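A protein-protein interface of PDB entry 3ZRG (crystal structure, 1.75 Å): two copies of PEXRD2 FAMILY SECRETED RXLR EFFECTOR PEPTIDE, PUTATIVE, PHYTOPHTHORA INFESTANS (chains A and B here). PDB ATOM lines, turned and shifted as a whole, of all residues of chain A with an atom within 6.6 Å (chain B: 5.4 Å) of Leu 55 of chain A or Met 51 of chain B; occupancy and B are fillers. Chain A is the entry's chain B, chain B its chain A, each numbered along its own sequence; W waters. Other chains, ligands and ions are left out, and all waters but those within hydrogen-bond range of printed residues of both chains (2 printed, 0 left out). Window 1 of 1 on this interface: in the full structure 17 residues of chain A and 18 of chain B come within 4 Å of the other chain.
Water W2 lies within hydrogen-bond range of the side-chain amino group of Lys 52 of chain A (2.7 Å) and the backbone carbonyl oxygen of Ala 35 of chain B (2.9 Å). Water W1 bridges the backbone carbonyl oxygen (O) of Met 42 of chain B (3.2 Å) and the backbone carbonyl oxygen (O) of Met 42 of chain A (3.2 Å).
Of the 17 printed residues of chain B, 8 touch a printed residue of chain A. Hydrophobic or aromatic side chains of chain B within 4 Å of the printed part of chain A: Ile 32, Ala 33, Ala 35, Ala 36, Met 42, Met 51 and Leu 55. Of the 14 printed residues of chain A, 7 touch a printed residue of chain B. Hydrophobic or aromatic side chains of chain A that line the printed part of chain B: Met 42, Met 51, Leu 55 and Leu 58.
NZ of Lys 52 of chain A sits at hydrogen-bond distance from O of Ala 36 of chain B, at 2.8 Å. The backbone carbonyl oxygen (O) of Ala 36 of chain B sits at hydrogen-bond distance from the guanidinium group (NH2) of Arg 56 of chain A (3.3 Å).
The side-chain hydroxyl (OG1) of Thr 48 of chain B is in hydrogen-bond range of the backbone NH (N) of Met 51 of chain B (3.1 Å).
Of the printed residues of chain B, Leu 55 of chain A touches Ile 32 (3.3 Å), Ala 35 (3.8 Å), Met 42 (3.7 Å) and Met 51 (3.8 Å). Printed residues of chain B within 4 Å of Arg 56 of chain A: Ala 36 (3.3 Å). Tyr 60 of chain A touches none of the printed residues of chain B. Met 51 of chain B touches one residue of chain A. Lys 53 of chain B touches none of the printed residues of chain A. Printed residues of chain A within 4 Å of Leu 55 of chain B: Met 42 (3.2 Å) and Met 51 (3.95 Å). The nearest residue of chain B that does not touch Leu 55 of chain A is Ala 36 of chain B (4.1 Å).
Met 42 of chain A touches Leu 55 of chain B, and with the chains exchanged Leu 55 of chain A touches Met 42 of chain B. Met 51 of chain A touches Leu 55 of chain B, and with the chains exchanged Leu 55 of chain A touches Met 51 of chain B. Lys 52 of chain A touches Met 42 of chain B, but with the chains exchanged Met 42 of chain A does not touch Lys 52 of chain B (5.3 Å). 8 positions are printed for both chains. Of the 12 pairs that touch across the chains among the printed residues, 4 have their exchanged pair printed and touching as well.
CG of Met 42 of chain A touches O of Gly 46 of chain B, at 3.5 Å. Leu 55 of chain B touches Met 42 of chain A. CE of Met 51 of chain A touches CD2 of Leu 55 of chain B, 3.95 Å away. Lys 52 of chain A touches Met 42 of chain B. Leu 55 of chain A touches Ile 32 of chain B. CD1 of Leu 55 of chain A touches CB of Ala 35 of chain B (3.8 Å). SD of Met 42 of chain B touches CD1 of Leu 55 of chain A, at 3.7 Å. Leu 55 of chain A touches Met 51 of chain B (CD2 to CE, 3.8 Å). CD2 of Leu 58 of chain A touches CD1 of Ile 32 of chain B, 3.9 Å away. CG of Asn 59 of chain A touches CB of Ala 33 of chain B, at 3.7 Å.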
ATOM      1  N   VAL A  19      -5.312  16.493 -18.038  1.00  0.00           N
ATOM      2  CA  VAL A  19      -4.297  16.298 -19.091  1.00  0.00           C
ATOM      3  C   VAL A  19      -3.451  15.066 -18.768  1.00  0.00           C
ATOM      4  O   VAL A  19      -3.190  14.242 -19.649  1.00  0.00           O
ATOM      5  CB  VAL A  19      -3.408  17.530 -19.255  1.00  0.00           C
ATOM      6  CG1 VAL A  19      -2.261  17.275 -20.236  1.00  0.00           C
ATOM      7  CG2 VAL A  19      -4.206  18.698 -19.811  1.00  0.00           C
ATOM      8  N   TYR A  22      -5.263  11.865 -19.420  1.00  0.00           N
ATOM      9  CA  TYR A  22      -5.285  11.564 -20.855  1.00  0.00           C
ATOM     10  C   TYR A  22      -3.970  10.949 -21.295  1.00  0.00           C
ATOM     11  O   TYR A  22      -3.987   9.979 -22.033  1.00  0.00           O
ATOM     12  CB  TYR A  22      -5.614  12.801 -21.676  1.00  0.00           C
ATOM     13  CG  TYR A  22      -5.865  12.525 -23.149  1.00  0.00           C
ATOM     14  CD1 TYR A  22      -6.603  11.434 -23.562  1.00  0.00           C
ATOM     15  CD2 TYR A  22      -5.321  13.370 -24.138  1.00  0.00           C
ATOM     16  CE1 TYR A  22      -6.865  11.211 -24.910  1.00  0.00           C
ATOM     17  CE2 TYR A  22      -5.583  13.153 -25.463  1.00  0.00           C
ATOM     18  CZ  TYR A  22      -6.322  12.083 -25.861  1.00  0.00           C
ATOM     19  OH  TYR A  22      -6.566  11.836 -27.208  1.00  0.00           O
ATOM     20  N   MET A  42      13.042  11.773 -27.768  1.00  0.00           N
ATOM     21  CA  MET A  42      12.082  12.853 -27.687  1.00  0.00           C
ATOM     22  C   MET A  42      11.557  13.224 -29.067  1.00  0.00           C
ATOM     23  O   MET A  42      10.353  13.435 -29.212  1.00  0.00           O
ATOM     24  CB  MET A  42      12.682  14.064 -26.972  1.00  0.00           C
ATOM     25  CG  MET A  42      11.704  15.191 -26.772  1.00  0.00           C
ATOM     26  SD  MET A  42      10.262  14.783 -25.703  1.00  0.00           S
ATOM     27  CE  MET A  42      10.224  16.211 -24.631  1.00  0.00           C
ATOM     28  N   LYS A  50      -0.150  10.025 -30.882  1.00  0.00           N
ATOM     29  CA  LYS A  50      -0.474  10.086 -29.443  1.00  0.00           C
ATOM     30  C   LYS A  50       0.037  11.354 -28.783  1.00  0.00           C
ATOM     31  O   LYS A  50      -0.708  12.033 -28.045  1.00  0.00           O
ATOM     32  CB  LYS A  50       0.068   8.858 -28.700  1.00  0.00           C
ATOM     33  CG  LYS A  50      -0.849   7.634 -28.777  1.00  0.00           C
ATOM     34  CD  LYS A  50      -0.238   6.442 -28.002  1.00  0.00           C
ATOM     35  CE  LYS A  50      -1.177   5.241 -27.973  1.00  0.00           C
ATOM     36  NZ  LYS A  50      -0.581   4.170 -27.137  1.00  0.00           N
ATOM     37  N   MET A  51       1.286  11.708 -29.041  1.00  0.00           N
ATOM     38  CA  MET A  51       1.805  12.925 -28.459  1.00  0.00           C
ATOM     39  C   MET A  51       1.079  14.160 -29.000  1.00  0.00           C
ATOM     40  O   MET A  51       0.779  15.106 -28.242  1.00  0.00           O
ATOM     41  CB  MET A  51       3.308  13.038 -28.644  1.00  0.00           C
ATOM     42  CG  MET A  51       3.910  14.134 -27.891  1.00  0.00           C
ATOM     43  SD  MET A  51       3.794  13.780 -26.094  1.00  0.00           S
ATOM     44  CE  MET A  51       5.007  14.930 -25.469  1.00  0.00           C
ATOM     45  N   LYS A  52       0.767  14.168 -30.286  1.00  0.00           N
ATOM     46  CA  LYS A  52       0.093  15.315 -30.863  1.00  0.00           C
ATOM     47  C   LYS A  52      -1.300  15.469 -30.213  1.00  0.00           C
ATOM     48  O   LYS A  52      -1.721  16.584 -29.935  1.00  0.00           O
ATOM     49  CB  LYS A  52       0.001  15.194 -32.375  1.00  0.00           C
ATOM     50  CG  LYS A  52       1.374  15.330 -33.114  1.00  0.00           C
ATOM     51  CD  LYS A  52       1.345  14.753 -34.527  1.00  0.00           C
ATOM     52  CE  LYS A  52       0.390  15.521 -35.459  1.00  0.00           C
ATOM     53  NZ  LYS A  52       0.888  16.911 -35.685  1.00  0.00           N
ATOM     54  N   LYS A  53      -2.000  14.355 -29.989  1.00  0.00           N
ATOM     55  CA  LYS A  53      -3.334  14.392 -29.350  1.00  0.00           C
ATOM     56  C   LYS A  53      -3.222  14.914 -27.928  1.00  0.00           C
ATOM     57  O   LYS A  53      -4.031  15.722 -27.483  1.00  0.00           O
ATOM     58  CB  LYS A  53      -4.006  13.000 -29.372  1.00  0.00           C
ATOM     59  CG  LYS A  53      -4.415  12.487 -30.764  1.00  0.00           C
ATOM     60  CD  LYS A  53      -4.529  10.989 -30.786  1.00  0.00           C
ATOM     61  CE  LYS A  53      -5.533  10.465 -29.811  1.00  0.00           C
ATOM     62  NZ  LYS A  53      -5.896   9.065 -30.153  1.00  0.00           N
ATOM     63  N   LEU A  54      -2.210  14.477 -27.208  1.00  0.00           N
ATOM     64  CA  LEU A  54      -1.990  14.933 -25.846  1.00  0.00           C
ATOM     65  C   LEU A  54      -1.795  16.440 -25.791  1.00  0.00           C
ATOM     66  O   LEU A  54      -2.434  17.126 -25.001  1.00  0.00           O
ATOM     67  CB  LEU A  54      -0.798  14.205 -25.224  1.00  0.00           C
ATOM     68  CG  LEU A  54      -0.452  14.610 -23.818  1.00  0.00           C
ATOM     69  CD1 LEU A  54      -1.691  14.377 -22.877  1.00  0.00           C
ATOM     70  CD2 LEU A  54       0.783  13.867 -23.350  1.00  0.00           C
ATOM     71  N   LEU A  55      -0.956  16.953 -26.670  1.00  0.00           N
ATOM     72  CA  LEU A  55      -0.696  18.391 -26.686  1.00  0.00           C
ATOM     73  C   LEU A  55      -1.934  19.208 -27.111  1.00  0.00           C
ATOM     74  O   LEU A  55      -2.178  20.285 -26.536  1.00  0.00           O
ATOM     75  CB  LEU A  55       0.509  18.756 -27.552  1.00  0.00           C
ATOM     76  CG  LEU A  55       1.876  18.244 -27.086  1.00  0.00           C
ATOM     77  CD1 LEU A  55       3.004  19.099 -27.700  1.00  0.00           C
ATOM     78  CD2 LEU A  55       1.980  18.202 -25.573  1.00  0.00           C
ATOM     79  N   ARG A  56      -2.733  18.680 -28.043  1.00  0.00           N
ATOM     80  CA  ARG A  56      -3.958  19.369 -28.462  1.00  0.00           C
ATOM     81  C   ARG A  56      -4.907  19.478 -27.269  1.00  0.00           C
ATOM     82  O   ARG A  56      -5.497  20.554 -27.021  1.00  0.00           O
ATOM     83  CB  ARG A  56      -4.666  18.605 -29.584  1.00  0.00           C
ATOM     84  CG  ARG A  56      -5.828  19.408 -30.209  1.00  0.00           C
ATOM     85  CD  ARG A  56      -6.358  18.756 -31.443  1.00  0.00           C
ATOM     86  NE  ARG A  56      -5.291  18.345 -32.347  1.00  0.00           N
ATOM     87  CZ  ARG A  56      -4.647  19.136 -33.202  1.00  0.00           C
ATOM     88  NH1 ARG A  56      -4.943  20.426 -33.347  1.00  0.00           N
ATOM     89  NH2 ARG A  56      -3.691  18.613 -33.959  1.00  0.00           N
ATOM     90  N   TYR A  57      -5.043  18.363 -26.542  1.00  0.00           N
ATOM     91  CA  TYR A  57      -5.918  18.307 -25.339  1.00  0.00           C
ATOM     92  C   TYR A  57      -5.417  19.254 -24.254  1.00  0.00           C
ATOM     93  O   TYR A  57      -6.215  19.994 -23.617  1.00  0.00           O
ATOM     94  CB  TYR A  57      -6.117  16.869 -24.818  1.00  0.00           C
ATOM     95  CG  TYR A  57      -7.239  16.776 -23.781  1.00  0.00           C
ATOM     96  CD1 TYR A  57      -8.530  17.261 -24.064  1.00  0.00           C
ATOM     97  CD2 TYR A  57      -7.008  16.253 -22.531  1.00  0.00           C
ATOM     98  CE1 TYR A  57      -9.557  17.181 -23.123  1.00  0.00           C
ATOM     99  CE2 TYR A  57      -8.019  16.170 -21.566  1.00  0.00           C
ATOM    100  CZ  TYR A  57      -9.288  16.645 -21.864  1.00  0.00           C
ATOM    101  OH  TYR A  57     -10.260  16.589 -20.897  1.00  0.00           O
ATOM    102  N   LEU A  58      -4.101  19.341 -24.080  1.00  0.00           N
ATOM    103  CA  LEU A  58      -3.549  20.245 -23.072  1.00  0.00           C
ATOM    104  C   LEU A  58      -3.987  21.672 -23.359  1.00  0.00           C
ATOM    105  O   LEU A  58      -4.475  22.379 -22.463  1.00  0.00           O
ATOM    106  CB  LEU A  58      -2.020  20.139 -23.028  1.00  0.00           C
ATOM    107  CG  LEU A  58      -1.281  20.901 -21.940  1.00  0.00           C
ATOM    108  CD1 LEU A  58       0.119  20.273 -21.806  1.00  0.00           C
ATOM    109  CD2 LEU A  58      -1.163  22.392 -22.227  1.00  0.00           C
ATOM    110  N   ASN A  59      -3.840  22.112 -24.606  1.00  0.00           N
ATOM    111  CA  ASN A  59      -4.279  23.454 -24.944  1.00  0.00           C
ATOM    112  C   ASN A  59      -5.814  23.603 -24.818  1.00  0.00           C
ATOM    113  O   ASN A  59      -6.270  24.608 -24.325  1.00  0.00           O
ATOM    114  CB  ASN A  59      -3.779  23.913 -26.339  1.00  0.00           C
ATOM    115  CG  ASN A  59      -4.222  25.331 -26.675  1.00  0.00           C
ATOM    116  OD1 ASN A  59      -3.724  26.308 -26.092  1.00  0.00           O
ATOM    117  ND2 ASN A  59      -5.178  25.454 -27.573  1.00  0.00           N
ATOM    118  N   TYR A  60      -6.566  22.605 -25.246  1.00  0.00           N
ATOM    119  CA  TYR A  60      -8.034  22.624 -25.094  1.00  0.00           C
ATOM    120  C   TYR A  60      -8.456  22.847 -23.619  1.00  0.00           C
ATOM    121  O   TYR A  60      -9.222  23.756 -23.329  1.00  0.00           O
ATOM    122  CB  TYR A  60      -8.649  21.335 -25.618  1.00  0.00           C
ATOM    123  CG  TYR A  60     -10.155  21.383 -25.610  1.00  0.00           C
ATOM    124  CD1 TYR A  60     -10.841  21.906 -26.675  1.00  0.00           C
ATOM    125  CD2 TYR A  60     -10.891  20.903 -24.522  1.00  0.00           C
ATOM    126  CE1 TYR A  60     -12.224  21.957 -26.668  1.00  0.00           C
ATOM    127  CE2 TYR A  60     -12.268  20.943 -24.510  1.00  0.00           C
ATOM    128  CZ  TYR A  60     -12.935  21.468 -25.554  1.00  0.00           C
ATOM    129  OH  TYR A  60     -14.325  21.524 -25.509  1.00  0.00           O
ATOM    130  N   LEU B  28       4.088  28.472 -22.156  1.00  0.00           N
ATOM    131  CA  LEU B  28       4.228  27.431 -23.146  1.00  0.00           C
ATOM    132  C   LEU B  28       2.908  27.052 -23.859  1.00  0.00           C
ATOM    133  O   LEU B  28       2.902  26.301 -24.816  1.00  0.00           O
ATOM    134  CB  LEU B  28       4.749  26.201 -22.432  1.00  0.00           C
ATOM    135  CG  LEU B  28       5.997  25.504 -22.953  1.00  0.00           C
ATOM    136  CD1 LEU B  28       7.110  26.435 -23.435  1.00  0.00           C
ATOM    137  CD2 LEU B  28       6.433  24.515 -21.908  1.00  0.00           C
ATOM    138  N   ILE B  32       2.613  24.987 -27.343  1.00  0.00           N
ATOM    139  CA  ILE B  32       2.030  23.627 -27.297  1.00  0.00           C
ATOM    140  C   ILE B  32       0.934  23.420 -28.326  1.00  0.00           C
ATOM    141  O   ILE B  32       0.876  22.357 -28.969  1.00  0.00           O
ATOM    142  CB  ILE B  32       1.548  23.275 -25.881  1.00  0.00           C
ATOM    143  CG1 ILE B  32       2.754  22.984 -24.988  1.00  0.00           C
ATOM    144  CG2 ILE B  32       0.591  22.030 -25.903  1.00  0.00           C
ATOM    145  CD1 ILE B  32       2.499  23.089 -23.466  1.00  0.00           C
ATOM    146  N   ALA B  33       0.076  24.430 -28.505  1.00  0.00           N
ATOM    147  CA  ALA B  33      -0.945  24.432 -29.519  1.00  0.00           C
ATOM    148  C   ALA B  33      -0.293  24.323 -30.886  1.00  0.00           C
ATOM    149  O   ALA B  33      -0.743  23.545 -31.739  1.00  0.00           O
ATOM    150  CB  ALA B  33      -1.824  25.705 -29.423  1.00  0.00           C
ATOM    151  N   ALA B  35       2.683  23.144 -31.620  1.00  0.00           N
ATOM    152  CA  ALA B  35       3.371  21.853 -31.690  1.00  0.00           C
ATOM    153  C   ALA B  35       2.417  20.712 -32.030  1.00  0.00           C
ATOM    154  O   ALA B  35       2.807  19.762 -32.704  1.00  0.00           O
ATOM    155  CB  ALA B  35       4.080  21.560 -30.376  1.00  0.00           C
ATOM    156  N   ALA B  36       1.174  20.768 -31.550  1.00  0.00           N
ATOM    157  CA  ALA B  36       0.187  19.720 -31.895  1.00  0.00           C
ATOM    158  C   ALA B  36      -0.077  19.656 -33.387  1.00  0.00           C
ATOM    159  O   ALA B  36      -0.436  18.605 -33.886  1.00  0.00           O
ATOM    160  CB  ALA B  36      -1.164  19.901 -31.093  1.00  0.00           C
ATOM    161  N   MET B  42       6.877  21.057 -32.996  1.00  0.00           N
ATOM    162  CA  MET B  42       6.992  19.978 -32.019  1.00  0.00           C
ATOM    163  C   MET B  42       8.435  19.630 -31.711  1.00  0.00           C
ATOM    164  O   MET B  42       8.819  19.497 -30.516  1.00  0.00           O
ATOM    165  CB  MET B  42       6.293  18.716 -32.543  1.00  0.00           C
ATOM    166  CG  MET B  42       6.402  17.503 -31.597  1.00  0.00           C
ATOM    167  SD  MET B  42       5.392  17.642 -30.086  1.00  0.00           S
ATOM    168  CE  MET B  42       3.828  17.110 -30.793  1.00  0.00           C
ATOM    169  N   LEU B  45      10.014  22.495 -29.733  1.00  0.00           N
ATOM    170  CA  LEU B  45       9.538  22.550 -28.366  1.00  0.00           C
ATOM    171  C   LEU B  45      10.161  21.415 -27.535  1.00  0.00           C
ATOM    172  O   LEU B  45      10.482  21.598 -26.366  1.00  0.00           O
ATOM    173  CB  LEU B  45       8.032  22.446 -28.340  1.00  0.00           C
ATOM    174  CG  LEU B  45       7.308  22.443 -26.989  1.00  0.00           C
ATOM    175  CD1 LEU B  45       7.510  23.686 -26.142  1.00  0.00           C
ATOM    176  CD2 LEU B  45       5.815  22.178 -27.239  1.00  0.00           C
ATOM    177  N   GLY B  46      10.328  20.257 -28.169  1.00  0.00           N
ATOM    178  CA  GLY B  46      10.821  19.055 -27.478  1.00  0.00           C
ATOM    179  C   GLY B  46      12.243  19.190 -27.015  1.00  0.00           C
ATOM    180  O   GLY B  46      12.649  18.480 -26.102  1.00  0.00           O
ATOM    181  N   THR B  48      13.402  21.894 -25.582  1.00  0.00           N
ATOM    182  CA  THR B  48      13.459  22.949 -24.563  1.00  0.00           C
ATOM    183  C   THR B  48      13.470  22.440 -23.121  1.00  0.00           C
ATOM    184  O   THR B  48      12.828  21.457 -22.802  1.00  0.00           O
ATOM    185  CB  THR B  48      12.318  23.972 -24.699  1.00  0.00           C
ATOM    186  OG1 THR B  48      11.060  23.343 -24.431  1.00  0.00           O
ATOM    187  CG2 THR B  48      12.356  24.635 -26.106  1.00  0.00           C
ATOM    188  N   LEU B  49      14.164  23.191 -22.267  1.00  0.00           N
ATOM    189  CA  LEU B  49      14.156  22.970 -20.821  1.00  0.00           C
ATOM    190  C   LEU B  49      12.726  23.114 -20.285  1.00  0.00           C
ATOM    191  O   LEU B  49      12.293  22.339 -19.439  1.00  0.00           O
ATOM    192  CB  LEU B  49      15.078  23.993 -20.153  1.00  0.00           C
ATOM    193  CG  LEU B  49      15.083  24.028 -18.627  1.00  0.00           C
ATOM    194  CD1 LEU B  49      15.351  22.627 -18.109  1.00  0.00           C
ATOM    195  CD2 LEU B  49      16.036  25.021 -18.044  1.00  0.00           C
ATOM    196  N   LYS B  50      11.985  24.079 -20.818  1.00  0.00           N
ATOM    197  CA  LYS B  50      10.610  24.295 -20.369  1.00  0.00           C
ATOM    198  C   LYS B  50       9.725  23.080 -20.601  1.00  0.00           C
ATOM    199  O   LYS B  50       8.952  22.695 -19.712  1.00  0.00           O
ATOM    200  CB  LYS B  50      10.022  25.539 -21.029  1.00  0.00           C
ATOM    201  CG  LYS B  50      10.482  26.799 -20.414  1.00  0.00           C
ATOM    202  CD  LYS B  50       9.942  27.991 -21.178  1.00  0.00           C
ATOM    203  CE  LYS B  50      10.125  29.272 -20.405  1.00  0.00           C
ATOM    204  NZ  LYS B  50       9.420  30.389 -21.082  1.00  0.00           N
ATOM    205  N   MET B  51       9.844  22.444 -21.767  1.00  0.00           N
ATOM    206  CA  MET B  51       9.035  21.245 -22.050  1.00  0.00           C
ATOM    207  C   MET B  51       9.470  20.065 -21.184  1.00  0.00           C
ATOM    208  O   MET B  51       8.636  19.282 -20.763  1.00  0.00           O
ATOM    209  CB  MET B  51       9.152  20.846 -23.514  1.00  0.00           C
ATOM    210  CG  MET B  51       8.154  19.824 -23.952  1.00  0.00           C
ATOM    211  SD  MET B  51       6.432  20.314 -23.700  1.00  0.00           S
ATOM    212  CE  MET B  51       5.546  19.055 -24.568  1.00  0.00           C
ATOM    213  N   LYS B  52      10.767  19.953 -20.935  1.00  0.00           N
ATOM    214  CA  LYS B  52      11.299  18.902 -20.063  1.00  0.00           C
ATOM    215  C   LYS B  52      10.650  19.022 -18.666  1.00  0.00           C
ATOM    216  O   LYS B  52      10.224  18.036 -18.093  1.00  0.00           O
ATOM    217  CB  LYS B  52      12.825  18.973 -19.984  1.00  0.00           C
ATOM    218  CG  LYS B  52      13.459  17.814 -19.175  1.00  0.00           C
ATOM    219  CD  LYS B  52      14.927  18.029 -18.916  1.00  0.00           C
ATOM    220  CE  LYS B  52      15.748  17.917 -20.163  1.00  0.00           C
ATOM    221  NZ  LYS B  52      15.745  16.552 -20.751  1.00  0.00           N
ATOM    222  N   LYS B  53      10.569  20.238 -18.147  1.00  0.00           N
ATOM    223  CA  LYS B  53       9.976  20.493 -16.848  1.00  0.00           C
ATOM    224  C   LYS B  53       8.504  20.176 -16.896  1.00  0.00           C
ATOM    225  O   LYS B  53       7.968  19.522 -15.990  1.00  0.00           O
ATOM    226  CB  LYS B  53      10.166  21.970 -16.428  1.00  0.00           C
ATOM    227  CG  LYS B  53      11.565  22.365 -15.951  1.00  0.00           C
ATOM    228  CD  LYS B  53      11.522  23.906 -15.659  1.00  0.00           C
ATOM    229  CE  LYS B  53      12.807  24.550 -15.318  1.00  0.00           C
ATOM    230  NZ  LYS B  53      12.465  25.969 -14.969  1.00  0.00           N
ATOM    231  N   LEU B  54       7.817  20.639 -17.942  1.00  0.00           N
ATOM    232  CA  LEU B  54       6.381  20.377 -18.064  1.00  0.00           C
ATOM    233  C   LEU B  54       6.037  18.866 -18.066  1.00  0.00           C
ATOM    234  O   LEU B  54       5.104  18.378 -17.371  1.00  0.00           O
ATOM    235  CB  LEU B  54       5.845  21.074 -19.310  1.00  0.00           C
ATOM    236  CG  LEU B  54       4.343  20.897 -19.519  1.00  0.00           C
ATOM    237  CD1 LEU B  54       3.480  21.467 -18.318  1.00  0.00           C
ATOM    238  CD2 LEU B  54       3.964  21.460 -20.875  1.00  0.00           C
ATOM    239  N   LEU B  55       6.809  18.108 -18.839  1.00  0.00           N
ATOM    240  CA  LEU B  55       6.558  16.678 -18.974  1.00  0.00           C
ATOM    241  C   LEU B  55       6.944  15.965 -17.669  1.00  0.00           C
ATOM    242  O   LEU B  55       6.312  14.994 -17.311  1.00  0.00           O
ATOM    243  CB  LEU B  55       7.316  16.132 -20.167  1.00  0.00           C
ATOM    244  CG  LEU B  55       6.747  16.571 -21.516  1.00  0.00           C
ATOM    245  CD1 LEU B  55       7.712  16.033 -22.612  1.00  0.00           C
ATOM    246  CD2 LEU B  55       5.291  16.089 -21.700  1.00  0.00           C
ATOM    247  N   ARG B  56       7.971  16.429 -16.960  1.00  0.00           N
ATOM    248  CA  ARG B  56       8.306  15.944 -15.630  1.00  0.00           C
ATOM    249  C   ARG B  56       7.121  16.058 -14.654  1.00  0.00           C
ATOM    250  O   ARG B  56       6.771  15.118 -13.932  1.00  0.00           O
ATOM    251  CB  ARG B  56       9.482  16.774 -15.099  1.00  0.00           C
ATOM    252  CG  ARG B  56      10.087  16.204 -13.862  1.00  0.00           C
ATOM    253  CD  ARG B  56      10.329  14.723 -14.062  1.00  0.00           C
ATOM    254  NE  ARG B  56      10.473  14.048 -12.790  1.00  0.00           N
ATOM    255  CZ  ARG B  56       9.541  13.278 -12.236  1.00  0.00           C
ATOM    256  NH1 ARG B  56       8.375  13.041 -12.867  1.00  0.00           N
ATOM    257  NH2 ARG B  56       9.808  12.730 -11.056  1.00  0.00           N
HETATM  258  O   HOH W   1       9.703  16.514 -29.984  1.00  0.00           O
HETATM  259  O   HOH W   2       3.264  17.884 -34.834  1.00  0.00           O
